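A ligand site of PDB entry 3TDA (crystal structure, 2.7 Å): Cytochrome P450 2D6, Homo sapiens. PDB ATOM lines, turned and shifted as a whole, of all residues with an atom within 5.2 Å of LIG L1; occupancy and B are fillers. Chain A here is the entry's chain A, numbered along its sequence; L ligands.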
ATOM      1  N   LEU A  88       4.862  -9.303  36.880  1.00  0.00           N
ATOM      2  CA  LEU A  88       5.505  -9.132  35.584  1.00  0.00           C
ATOM      3  C   LEU A  88       6.621  -8.062  35.611  1.00  0.00           C
ATOM      4  O   LEU A  88       7.153  -7.667  34.567  1.00  0.00           O
ATOM      5  CB  LEU A  88       4.435  -8.773  34.554  1.00  0.00           C
ATOM      6  CG  LEU A  88       3.146  -9.617  34.607  1.00  0.00           C
ATOM      7  CD1 LEU A  88       2.058  -9.052  33.686  1.00  0.00           C
ATOM      8  CD2 LEU A  88       3.492 -11.020  34.189  1.00  0.00           C
ATOM      9  N   PHE A  90       6.200  -4.991  36.980  1.00  0.00           N
ATOM     10  CA  PHE A  90       5.626  -3.644  36.975  1.00  0.00           C
ATOM     11  C   PHE A  90       5.988  -2.924  38.263  1.00  0.00           C
ATOM     12  O   PHE A  90       5.853  -3.501  39.343  1.00  0.00           O
ATOM     13  CB  PHE A  90       4.092  -3.704  36.881  1.00  0.00           C
ATOM     14  CG  PHE A  90       3.563  -3.765  35.474  1.00  0.00           C
ATOM     15  CD1 PHE A  90       2.891  -2.674  34.925  1.00  0.00           C
ATOM     16  CD2 PHE A  90       3.709  -4.936  34.710  1.00  0.00           C
ATOM     17  CE1 PHE A  90       2.351  -2.750  33.638  1.00  0.00           C
ATOM     18  CE2 PHE A  90       3.182  -5.022  33.428  1.00  0.00           C
ATOM     19  CZ  PHE A  90       2.498  -3.931  32.891  1.00  0.00           C
ATOM     20  N   PHE A  98      -0.015   0.464  27.991  1.00  0.00           N
ATOM     21  CA  PHE A  98      -1.398   0.049  28.102  1.00  0.00           C
ATOM     22  C   PHE A  98      -1.969  -0.006  29.522  1.00  0.00           C
ATOM     23  O   PHE A  98      -3.043   0.514  29.771  1.00  0.00           O
ATOM     24  CB  PHE A  98      -1.549  -1.307  27.421  1.00  0.00           C
ATOM     25  CG  PHE A  98      -2.977  -1.704  27.159  1.00  0.00           C
ATOM     26  CD1 PHE A  98      -3.676  -1.181  26.078  1.00  0.00           C
ATOM     27  CD2 PHE A  98      -3.606  -2.651  27.973  1.00  0.00           C
ATOM     28  CE1 PHE A  98      -4.992  -1.606  25.798  1.00  0.00           C
ATOM     29  CE2 PHE A  98      -4.912  -3.084  27.711  1.00  0.00           C
ATOM     30  CZ  PHE A  98      -5.609  -2.564  26.616  1.00  0.00           C
ATOM     31  N   LEU A  99      -1.261  -0.628  30.452  1.00  0.00           N
ATOM     32  CA  LEU A  99      -1.751  -0.744  31.834  1.00  0.00           C
ATOM     33  C   LEU A  99      -1.188   0.327  32.733  1.00  0.00           C
ATOM     34  O   LEU A  99      -1.521   0.393  33.906  1.00  0.00           O
ATOM     35  CB  LEU A  99      -1.393  -2.099  32.408  1.00  0.00           C
ATOM     36  CG  LEU A  99      -2.210  -3.249  31.817  1.00  0.00           C
ATOM     37  CD1 LEU A  99      -1.734  -4.580  32.391  1.00  0.00           C
ATOM     38  CD2 LEU A  99      -3.686  -3.003  32.146  1.00  0.00           C
ATOM     39  N   ALA A 187       0.567 -15.250  23.730  1.00  0.00           N
ATOM     40  CA  ALA A 187      -0.110 -13.969  23.665  1.00  0.00           C
ATOM     41  C   ALA A 187      -1.615 -14.136  23.623  1.00  0.00           C
ATOM     42  O   ALA A 187      -2.354 -13.398  24.295  1.00  0.00           O
ATOM     43  CB  ALA A 187       0.362 -13.177  22.450  1.00  0.00           C
ATOM     44  N   GLY A 190      -2.913 -15.726  27.195  1.00  0.00           N
ATOM     45  CA  GLY A 190      -2.962 -14.700  28.209  1.00  0.00           C
ATOM     46  C   GLY A 190      -4.107 -13.711  28.040  1.00  0.00           C
ATOM     47  O   GLY A 190      -4.469 -12.987  28.963  1.00  0.00           O
ATOM     48  N   LEU A 191      -4.683 -13.672  26.844  1.00  0.00           N
ATOM     49  CA  LEU A 191      -5.799 -12.768  26.589  1.00  0.00           C
ATOM     50  C   LEU A 191      -7.052 -13.401  27.172  1.00  0.00           C
ATOM     51  O   LEU A 191      -8.164 -12.885  27.026  1.00  0.00           O
ATOM     52  CB  LEU A 191      -5.970 -12.546  25.087  1.00  0.00           C
ATOM     53  CG  LEU A 191      -6.730 -11.269  24.765  1.00  0.00           C
ATOM     54  CD1 LEU A 191      -5.991 -10.081  25.334  1.00  0.00           C
ATOM     55  CD2 LEU A 191      -6.889 -11.141  23.265  1.00  0.00           C
ATOM     56  N   GLU A 194      -6.722 -12.126  31.379  1.00  0.00           N
ATOM     57  CA  GLU A 194      -7.207 -10.782  31.684  1.00  0.00           C
ATOM     58  C   GLU A 194      -8.682 -10.859  32.112  1.00  0.00           C
ATOM     59  O   GLU A 194      -9.230  -9.915  32.693  1.00  0.00           O
ATOM     60  CB  GLU A 194      -7.071  -9.865  30.457  1.00  0.00           C
ATOM     61  CG  GLU A 194      -5.682  -9.281  30.225  1.00  0.00           C
ATOM     62  CD  GLU A 194      -5.451  -7.994  30.980  1.00  0.00           C
ATOM     63  OE1 GLU A 194      -6.076  -6.972  30.610  1.00  0.00           O
ATOM     64  OE2 GLU A 194      -4.661  -7.996  31.937  1.00  0.00           O
ATOM     65  N   GLN A 222       1.114 -14.580  30.525  1.00  0.00           N
ATOM     66  CA  GLN A 222       1.815 -13.315  30.362  1.00  0.00           C
ATOM     67  C   GLN A 222       3.266 -13.506  30.775  1.00  0.00           C
ATOM     68  O   GLN A 222       4.165 -12.930  30.154  1.00  0.00           O
ATOM     69  CB  GLN A 222       1.197 -12.200  31.208  1.00  0.00           C
ATOM     70  CG  GLN A 222       0.117 -11.381  30.531  1.00  0.00           C
ATOM     71  CD  GLN A 222      -1.253 -12.006  30.679  1.00  0.00           C
ATOM     72  OE1 GLN A 222      -1.608 -12.437  31.769  1.00  0.00           O
ATOM     73  NE2 GLN A 222      -2.030 -12.049  29.602  1.00  0.00           N
ATOM     74  N   PHE A 225       4.930 -15.476  28.135  1.00  0.00           N
ATOM     75  CA  PHE A 225       5.116 -14.533  27.050  1.00  0.00           C
ATOM     76  C   PHE A 225       6.376 -13.694  27.274  1.00  0.00           C
ATOM     77  O   PHE A 225       7.255 -13.642  26.414  1.00  0.00           O
ATOM     78  CB  PHE A 225       3.907 -13.604  26.928  1.00  0.00           C
ATOM     79  CG  PHE A 225       3.910 -12.772  25.677  1.00  0.00           C
ATOM     80  CD1 PHE A 225       3.654 -13.350  24.447  1.00  0.00           C
ATOM     81  CD2 PHE A 225       4.297 -11.455  25.715  1.00  0.00           C
ATOM     82  CE1 PHE A 225       3.793 -12.611  23.277  1.00  0.00           C
ATOM     83  CE2 PHE A 225       4.436 -10.716  24.545  1.00  0.00           C
ATOM     84  CZ  PHE A 225       4.190 -11.297  23.324  1.00  0.00           C
ATOM     85  N   LEU A 226       6.482 -13.054  28.427  1.00  0.00           N
ATOM     86  CA  LEU A 226       7.640 -12.221  28.731  1.00  0.00           C
ATOM     87  C   LEU A 226       8.932 -13.026  28.785  1.00  0.00           C
ATOM     88  O   LEU A 226       9.994 -12.543  28.361  1.00  0.00           O
ATOM     89  CB  LEU A 226       7.435 -11.476  30.058  1.00  0.00           C
ATOM     90  CG  LEU A 226       6.315 -10.434  30.013  1.00  0.00           C
ATOM     91  CD1 LEU A 226       6.150  -9.781  31.354  1.00  0.00           C
ATOM     92  CD2 LEU A 226       6.631  -9.393  28.948  1.00  0.00           C
ATOM     93  N   ILE A 275       8.529  -4.926  29.267  1.00  0.00           N
ATOM     94  CA  ILE A 275       7.114  -4.596  29.342  1.00  0.00           C
ATOM     95  C   ILE A 275       6.707  -3.752  28.130  1.00  0.00           C
ATOM     96  O   ILE A 275       5.726  -4.057  27.472  1.00  0.00           O
ATOM     97  CB  ILE A 275       6.755  -3.833  30.625  1.00  0.00           C
ATOM     98  CG1 ILE A 275       6.951  -4.749  31.834  1.00  0.00           C
ATOM     99  CG2 ILE A 275       5.297  -3.334  30.557  1.00  0.00           C
ATOM    100  CD1 ILE A 275       6.780  -4.055  33.142  1.00  0.00           C
ATOM    101  N   ALA A 278       6.759  -5.826  24.988  1.00  0.00           N
ATOM    102  CA  ALA A 278       5.695  -6.822  25.004  1.00  0.00           C
ATOM    103  C   ALA A 278       4.362  -6.134  24.824  1.00  0.00           C
ATOM    104  O   ALA A 278       3.391  -6.690  24.308  1.00  0.00           O
ATOM    105  CB  ALA A 278       5.697  -7.564  26.308  1.00  0.00           C
ATOM    106  N   ASP A 279       4.307  -4.891  25.269  1.00  0.00           N
ATOM    107  CA  ASP A 279       3.093  -4.099  25.194  1.00  0.00           C
ATOM    108  C   ASP A 279       2.707  -3.856  23.731  1.00  0.00           C
ATOM    109  O   ASP A 279       1.593  -4.152  23.314  1.00  0.00           O
ATOM    110  CB  ASP A 279       3.339  -2.768  25.904  1.00  0.00           C
ATOM    111  CG  ASP A 279       2.089  -2.176  26.468  1.00  0.00           C
ATOM    112  OD1 ASP A 279       1.216  -1.838  25.652  1.00  0.00           O
ATOM    113  OD2 ASP A 279       1.974  -2.057  27.702  1.00  0.00           O
ATOM    114  N   LEU A 280       3.670  -3.358  22.970  1.00  0.00           N
ATOM    115  CA  LEU A 280       3.466  -3.040  21.572  1.00  0.00           C
ATOM    116  C   LEU A 280       3.311  -4.289  20.710  1.00  0.00           C
ATOM    117  O   LEU A 280       2.433  -4.350  19.834  1.00  0.00           O
ATOM    118  CB  LEU A 280       4.632  -2.166  21.086  1.00  0.00           C
ATOM    119  CG  LEU A 280       4.799  -0.840  21.865  1.00  0.00           C
ATOM    120  CD1 LEU A 280       5.943  -0.013  21.307  1.00  0.00           C
ATOM    121  CD2 LEU A 280       3.536  -0.018  21.797  1.00  0.00           C
ATOM    122  N   SER A 282       2.396  -7.483  21.643  1.00  0.00           N
ATOM    123  CA  SER A 282       1.146  -8.176  21.865  1.00  0.00           C
ATOM    124  C   SER A 282      -0.029  -7.395  21.284  1.00  0.00           C
ATOM    125  O   SER A 282      -0.891  -7.953  20.625  1.00  0.00           O
ATOM    126  CB  SER A 282       0.922  -8.431  23.369  1.00  0.00           C
ATOM    127  OG  SER A 282       0.641  -7.229  24.074  1.00  0.00           O
ATOM    128  N   ALA A 283      -0.054  -6.090  21.521  1.00  0.00           N
ATOM    129  CA  ALA A 283      -1.148  -5.284  20.998  1.00  0.00           C
ATOM    130  C   ALA A 283      -1.220  -5.438  19.469  1.00  0.00           C
ATOM    131  O   ALA A 283      -2.300  -5.531  18.892  1.00  0.00           O
ATOM    132  CB  ALA A 283      -0.935  -3.836  21.395  1.00  0.00           C
ATOM    133  N   VAL A 286      -2.737  -9.087  17.870  1.00  0.00           N
ATOM    134  CA  VAL A 286      -4.097  -9.553  18.159  1.00  0.00           C
ATOM    135  C   VAL A 286      -5.230  -8.574  17.810  1.00  0.00           C
ATOM    136  O   VAL A 286      -6.398  -8.851  18.020  1.00  0.00           O
ATOM    137  CB  VAL A 286      -4.214  -9.926  19.673  1.00  0.00           C
ATOM    138  CG1 VAL A 286      -4.197  -8.664  20.545  1.00  0.00           C
ATOM    139  CG2 VAL A 286      -5.511 -10.691  19.911  1.00  0.00           C
ATOM    140  N   THR A 287      -4.879  -7.410  17.282  1.00  0.00           N
ATOM    141  CA  THR A 287      -5.881  -6.408  16.920  1.00  0.00           C
ATOM    142  C   THR A 287      -6.188  -6.366  15.430  1.00  0.00           C
ATOM    143  O   THR A 287      -7.263  -6.776  15.002  1.00  0.00           O
ATOM    144  CB  THR A 287      -5.419  -5.023  17.344  1.00  0.00           C
ATOM    145  OG1 THR A 287      -4.103  -4.778  16.798  1.00  0.00           O
ATOM    146  CG2 THR A 287      -5.420  -4.919  18.880  1.00  0.00           C
ATOM    147  N   VAL A 348     -13.414  -4.267  19.836  1.00  0.00           N
ATOM    148  CA  VAL A 348     -13.165  -3.916  21.222  1.00  0.00           C
ATOM    149  C   VAL A 348     -14.423  -3.205  21.704  1.00  0.00           C
ATOM    150  O   VAL A 348     -14.412  -2.012  21.944  1.00  0.00           O
ATOM    151  CB  VAL A 348     -11.981  -2.964  21.340  1.00  0.00           C
ATOM    152  CG1 VAL A 348     -11.534  -2.874  22.777  1.00  0.00           C
ATOM    153  CG2 VAL A 348     -10.855  -3.443  20.463  1.00  0.00           C
ATOM    154  N   CYS A 421      -5.815   4.740  21.362  1.00  0.00           N
ATOM    155  CA  CYS A 421      -4.863   3.798  20.774  1.00  0.00           C
ATOM    156  C   CYS A 421      -3.744   4.515  20.104  1.00  0.00           C
ATOM    157  O   CYS A 421      -3.995   5.395  19.270  1.00  0.00           O
ATOM    158  CB  CYS A 421      -5.547   2.913  19.744  1.00  0.00           C
ATOM    159  SG  CYS A 421      -4.487   1.563  19.109  1.00  0.00           S
ATOM    160  N   PHE A 461     -13.141  -9.673  25.605  1.00  0.00           N
ATOM    161  CA  PHE A 461     -12.621  -8.316  25.663  1.00  0.00           C
ATOM    162  C   PHE A 461     -12.252  -7.881  24.250  1.00  0.00           C
ATOM    163  O   PHE A 461     -12.524  -6.761  23.849  1.00  0.00           O
ATOM    164  CB  PHE A 461     -11.412  -8.241  26.598  1.00  0.00           C
ATOM    165  CG  PHE A 461     -10.463  -7.129  26.270  1.00  0.00           C
ATOM    166  CD1 PHE A 461     -10.773  -5.821  26.561  1.00  0.00           C
ATOM    167  CD2 PHE A 461      -9.243  -7.396  25.690  1.00  0.00           C
ATOM    168  CE1 PHE A 461      -9.899  -4.807  26.281  1.00  0.00           C
ATOM    169  CE2 PHE A 461      -8.357  -6.384  25.397  1.00  0.00           C
ATOM    170  CZ  PHE A 461      -8.687  -5.080  25.687  1.00  0.00           C
ATOM    171  N   LEU A 462     -11.650  -8.799  23.509  1.00  0.00           N
ATOM    172  CA  LEU A 462     -11.343  -8.596  22.113  1.00  0.00           C
ATOM    173  C   LEU A 462     -12.296  -9.518  21.357  1.00  0.00           C
ATOM    174  O   LEU A 462     -12.235 -10.729  21.523  1.00  0.00           O
ATOM    175  CB  LEU A 462      -9.893  -9.010  21.894  1.00  0.00           C
ATOM    176  CG  LEU A 462      -9.034  -8.194  20.952  1.00  0.00           C
ATOM    177  CD1 LEU A 462      -9.724  -8.122  19.604  1.00  0.00           C
ATOM    178  CD2 LEU A 462      -8.824  -6.823  21.536  1.00  0.00           C
HETATM  179  N1  LIG L   1      -0.813  -7.679  28.276  1.00  0.00           N
HETATM  180  N2  LIG L   1      -0.345  -5.228  26.031  1.00  0.00           N
HETATM  181  C1  LIG L   1       0.077  -7.597  30.652  1.00  0.00           C
HETATM  182  C2  LIG L   1      -2.814  -7.691  26.281  1.00  0.00           C
HETATM  183  C3  LIG L   1      -3.746  -6.785  26.859  1.00  0.00           C
HETATM  184  C4  LIG L   1      -4.609  -6.072  26.022  1.00  0.00           C
HETATM  185  C5  LIG L   1      -4.540  -6.263  24.606  1.00  0.00           C
HETATM  186  C6  LIG L   1      -2.729  -7.865  24.864  1.00  0.00           C
HETATM  187  C7  LIG L   1      -6.303  -2.913  21.664  1.00  0.00           C
HETATM  188  C8  LIG L   1      -3.984  -3.667  23.026  1.00  0.00           C
HETATM  189  C9  LIG L   1       2.823  -6.450  27.772  1.00  0.00           C
HETATM  190  C10 LIG L   1       1.653  -7.181  28.459  1.00  0.00           C
HETATM  191  C11 LIG L   1       0.333  -6.992  27.612  1.00  0.00           C
HETATM  192  C12 LIG L   1      -1.144  -7.486  29.722  1.00  0.00           C
HETATM  193  S1  LIG L   1       1.499  -6.611  30.145  1.00  0.00           S
HETATM  194  S2  LIG L   1      -1.798  -8.593  27.329  1.00  0.00           S
HETATM  195  C13 LIG L   1      -3.594  -7.148  24.040  1.00  0.00           C
HETATM  196  O1  LIG L   1      -5.385  -5.623  23.760  1.00  0.00           O
HETATM  197  C14 LIG L   1      -5.181  -4.472  23.100  1.00  0.00           C
HETATM  198  C15 LIG L   1      -6.338  -4.086  22.424  1.00  0.00           C
HETATM  199  N3  LIG L   1      -5.191  -2.141  21.584  1.00  0.00           N
HETATM  200  C16 LIG L   1      -4.058  -2.499  22.242  1.00  0.00           C
HETATM  201  O2  LIG L   1      -2.743  -9.228  28.206  1.00  0.00           O
HETATM  202  O3  LIG L   1      -0.943  -9.452  26.513  1.00  0.00           O
HETATM  203  C17 LIG L   1      -0.051  -5.523  27.315  1.00  0.00           C
HETATM  204  O4  LIG L   1      -0.714  -3.935  25.595  1.00  0.00           O
HETATM  205  O5  LIG L   1      -0.089  -4.671  28.224  1.00  0.00           O
HETATM  206  C18 LIG L   1       2.071  -8.672  28.405  1.00  0.00           C
HETATM  207  C1  LG2 L   2      -5.086   1.258  23.309  1.00  0.00           C
HETATM  208  C2  LG2 L   2      -8.052  -0.273  19.939  1.00  0.00           C
HETATM  209  C3  LG2 L   2      -4.356  -1.647  17.385  1.00  0.00           C
HETATM  210  C4  LG2 L   2      -1.410  -0.235  20.803  1.00  0.00           C
HETATM  211  C5  LG2 L   2      -6.261   1.113  22.588  1.00  0.00           C
HETATM  212  C6  LG2 L   2      -7.562   1.321  23.087  1.00  0.00           C
HETATM  213  C7  LG2 L   2      -8.411   0.801  22.149  1.00  0.00           C
HETATM  214  C8  LG2 L   2      -7.603   0.305  21.106  1.00  0.00           C
HETATM  215  C9  LG2 L   2      -9.991   0.771  22.224  1.00  0.00           C
HETATM  216  C10 LG2 L   2      -7.924   1.983  24.415  1.00  0.00           C
HETATM  217  C11 LG2 L   2      -8.114   3.457  24.407  1.00  0.00           C
HETATM  218  C12 LG2 L   2      -8.540   3.969  25.776  1.00  0.00           C
HETATM  219  O1  LG2 L   2      -7.881   3.708  26.780  1.00  0.00           O
HETATM  220  O2  LG2 L   2      -9.586   4.608  25.897  1.00  0.00           O
HETATM  221  C13 LG2 L   2      -7.366  -0.867  18.899  1.00  0.00           C
HETATM  222  C14 LG2 L   2      -7.909  -1.366  17.676  1.00  0.00           C
HETATM  223  C15 LG2 L   2      -6.787  -1.798  16.920  1.00  0.00           C
HETATM  224  C16 LG2 L   2      -5.667  -1.508  17.752  1.00  0.00           C
HETATM  225  C17 LG2 L   2      -9.364  -1.420  17.328  1.00  0.00           C
HETATM  226  C18 LG2 L   2      -6.719  -2.371  15.639  1.00  0.00           C
HETATM  227  C19 LG2 L   2      -7.613  -2.266  14.478  1.00  0.00           C
HETATM  228  C20 LG2 L   2      -3.174  -1.626  18.115  1.00  0.00           C
HETATM  229  C21 LG2 L   2      -1.897  -1.650  17.539  1.00  0.00           C
HETATM  230  C22 LG2 L   2      -1.023  -1.153  18.487  1.00  0.00           C
HETATM  231  C23 LG2 L   2      -1.818  -0.842  19.605  1.00  0.00           C
HETATM  232  C24 LG2 L   2      -1.538  -2.144  16.089  1.00  0.00           C
HETATM  233  C25 LG2 L   2       0.352  -0.951  18.425  1.00  0.00           C
HETATM  234  C26 LG2 L   2       1.403  -1.647  19.024  1.00  0.00           C
HETATM  235  C27 LG2 L   2      -2.145   0.215  21.839  1.00  0.00           C
HETATM  236  C28 LG2 L   2      -1.611   0.785  23.000  1.00  0.00           C
HETATM  237  C29 LG2 L   2      -2.659   1.263  23.735  1.00  0.00           C
HETATM  238  C30 LG2 L   2      -3.799   0.941  22.966  1.00  0.00           C
HETATM  239  C31 LG2 L   2      -0.119   0.871  23.413  1.00  0.00           C
HETATM  240  C32 LG2 L   2      -2.597   1.990  25.104  1.00  0.00           C
HETATM  241  C33 LG2 L   2      -2.481   3.533  24.990  1.00  0.00           C
HETATM  242  C34 LG2 L   2      -2.411   4.339  26.312  1.00  0.00           C
HETATM  243  O3  LG2 L   2      -1.890   5.424  26.361  1.00  0.00           O
HETATM  244  O4  LG2 L   2      -2.922   3.863  27.320  1.00  0.00           O
HETATM  245  N1  LG2 L   2      -6.323   0.487  21.372  1.00  0.00           N
HETATM  246  N2  LG2 L   2      -6.033  -0.969  18.903  1.00  0.00           N
HETATM  247  N3  LG2 L   2      -3.135  -1.140  19.354  1.00  0.00           N
HETATM  248  N4  LG2 L   2      -3.449   0.318  21.848  1.00  0.00           N
HETATM  249 FE1  LG2 L   2      -4.745  -0.370  20.367  1.00  0.00          FE
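The side-chain hydroxyl (OG) of Ser 282 sits at hydrogen-bond distance from a nitrogen (N2) of LIG L1 (3.0 Å). O2 of LIG L1 is in hydrogen-bond range of NE2 of Gln 222 (3.2 Å). An iron atom (FE1) of LG2 L2 is bound by the side-chain sulfur of Cys 421, at 2.3 Å. O of Asp 279 is in hydrogen-bond range of O4 of LIG L1. OD1 of Asp 279 sits at hydrogen-bond distance from O4 of LIG L1, at 2.9 Å.
A nitrogen (N3) of LIG L1 binds an iron atom (FE1) of LG2 L2 (2.2 Å).
OD2 of Asp 279 lies within hydrogen-bond range of N of Phe 98 (3.2 Å). The side-chain amide nitrogen of Gln 222 sits at hydrogen-bond distance from the backbone carbonyl oxygen of Gly 190 (2.7 Å). OG of Ser 282 is in hydrogen-bond range of O of Asp 279. The side-chain hydroxyl of Ser 282 sits at hydrogen-bond distance from the backbone carbonyl oxygen of Ala 278, at 2.8 Å. OG1 of Thr 287 lies within hydrogen-bond range of O of Ala 283.
Merely in contact with LIG L1: Phe 98 (3.3 Å), Ala 278 (3.3 Å), Ala 283 (3.5 Å), Phe 461 (3.5 Å), Thr 287 (3.5 Å), Glu 194 (3.6 Å), Ile 275 (3.8 Å), Leu 462 (3.8 Å), Val 286 (3.9 Å), Leu 88 (3.9 Å), Leu 99 (3.9 Å), Phe 90 (3.96 Å) and Leu 191 (3.97 Å). Hydrophobic or aromatic side chains within 4 Å of LIG L1: Leu 88, Phe 90, Phe 98, Leu 99, Leu 191, Ala 278, Ala 283, Val 286, Phe 461 and Leu 462. Within 4 Å of LIG L1: Leu 88, Phe 90, Phe 98, Leu 99, Leu 191, Glu 194, Gln 222, Ile 275, Ala 278, Asp 279, Ser 282, Ala 283, Val 286, Thr 287, Phe 461 and Leu 462. The nearest printed residue that does not touch LIG L1 is Gly 190 (4.2 Å).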
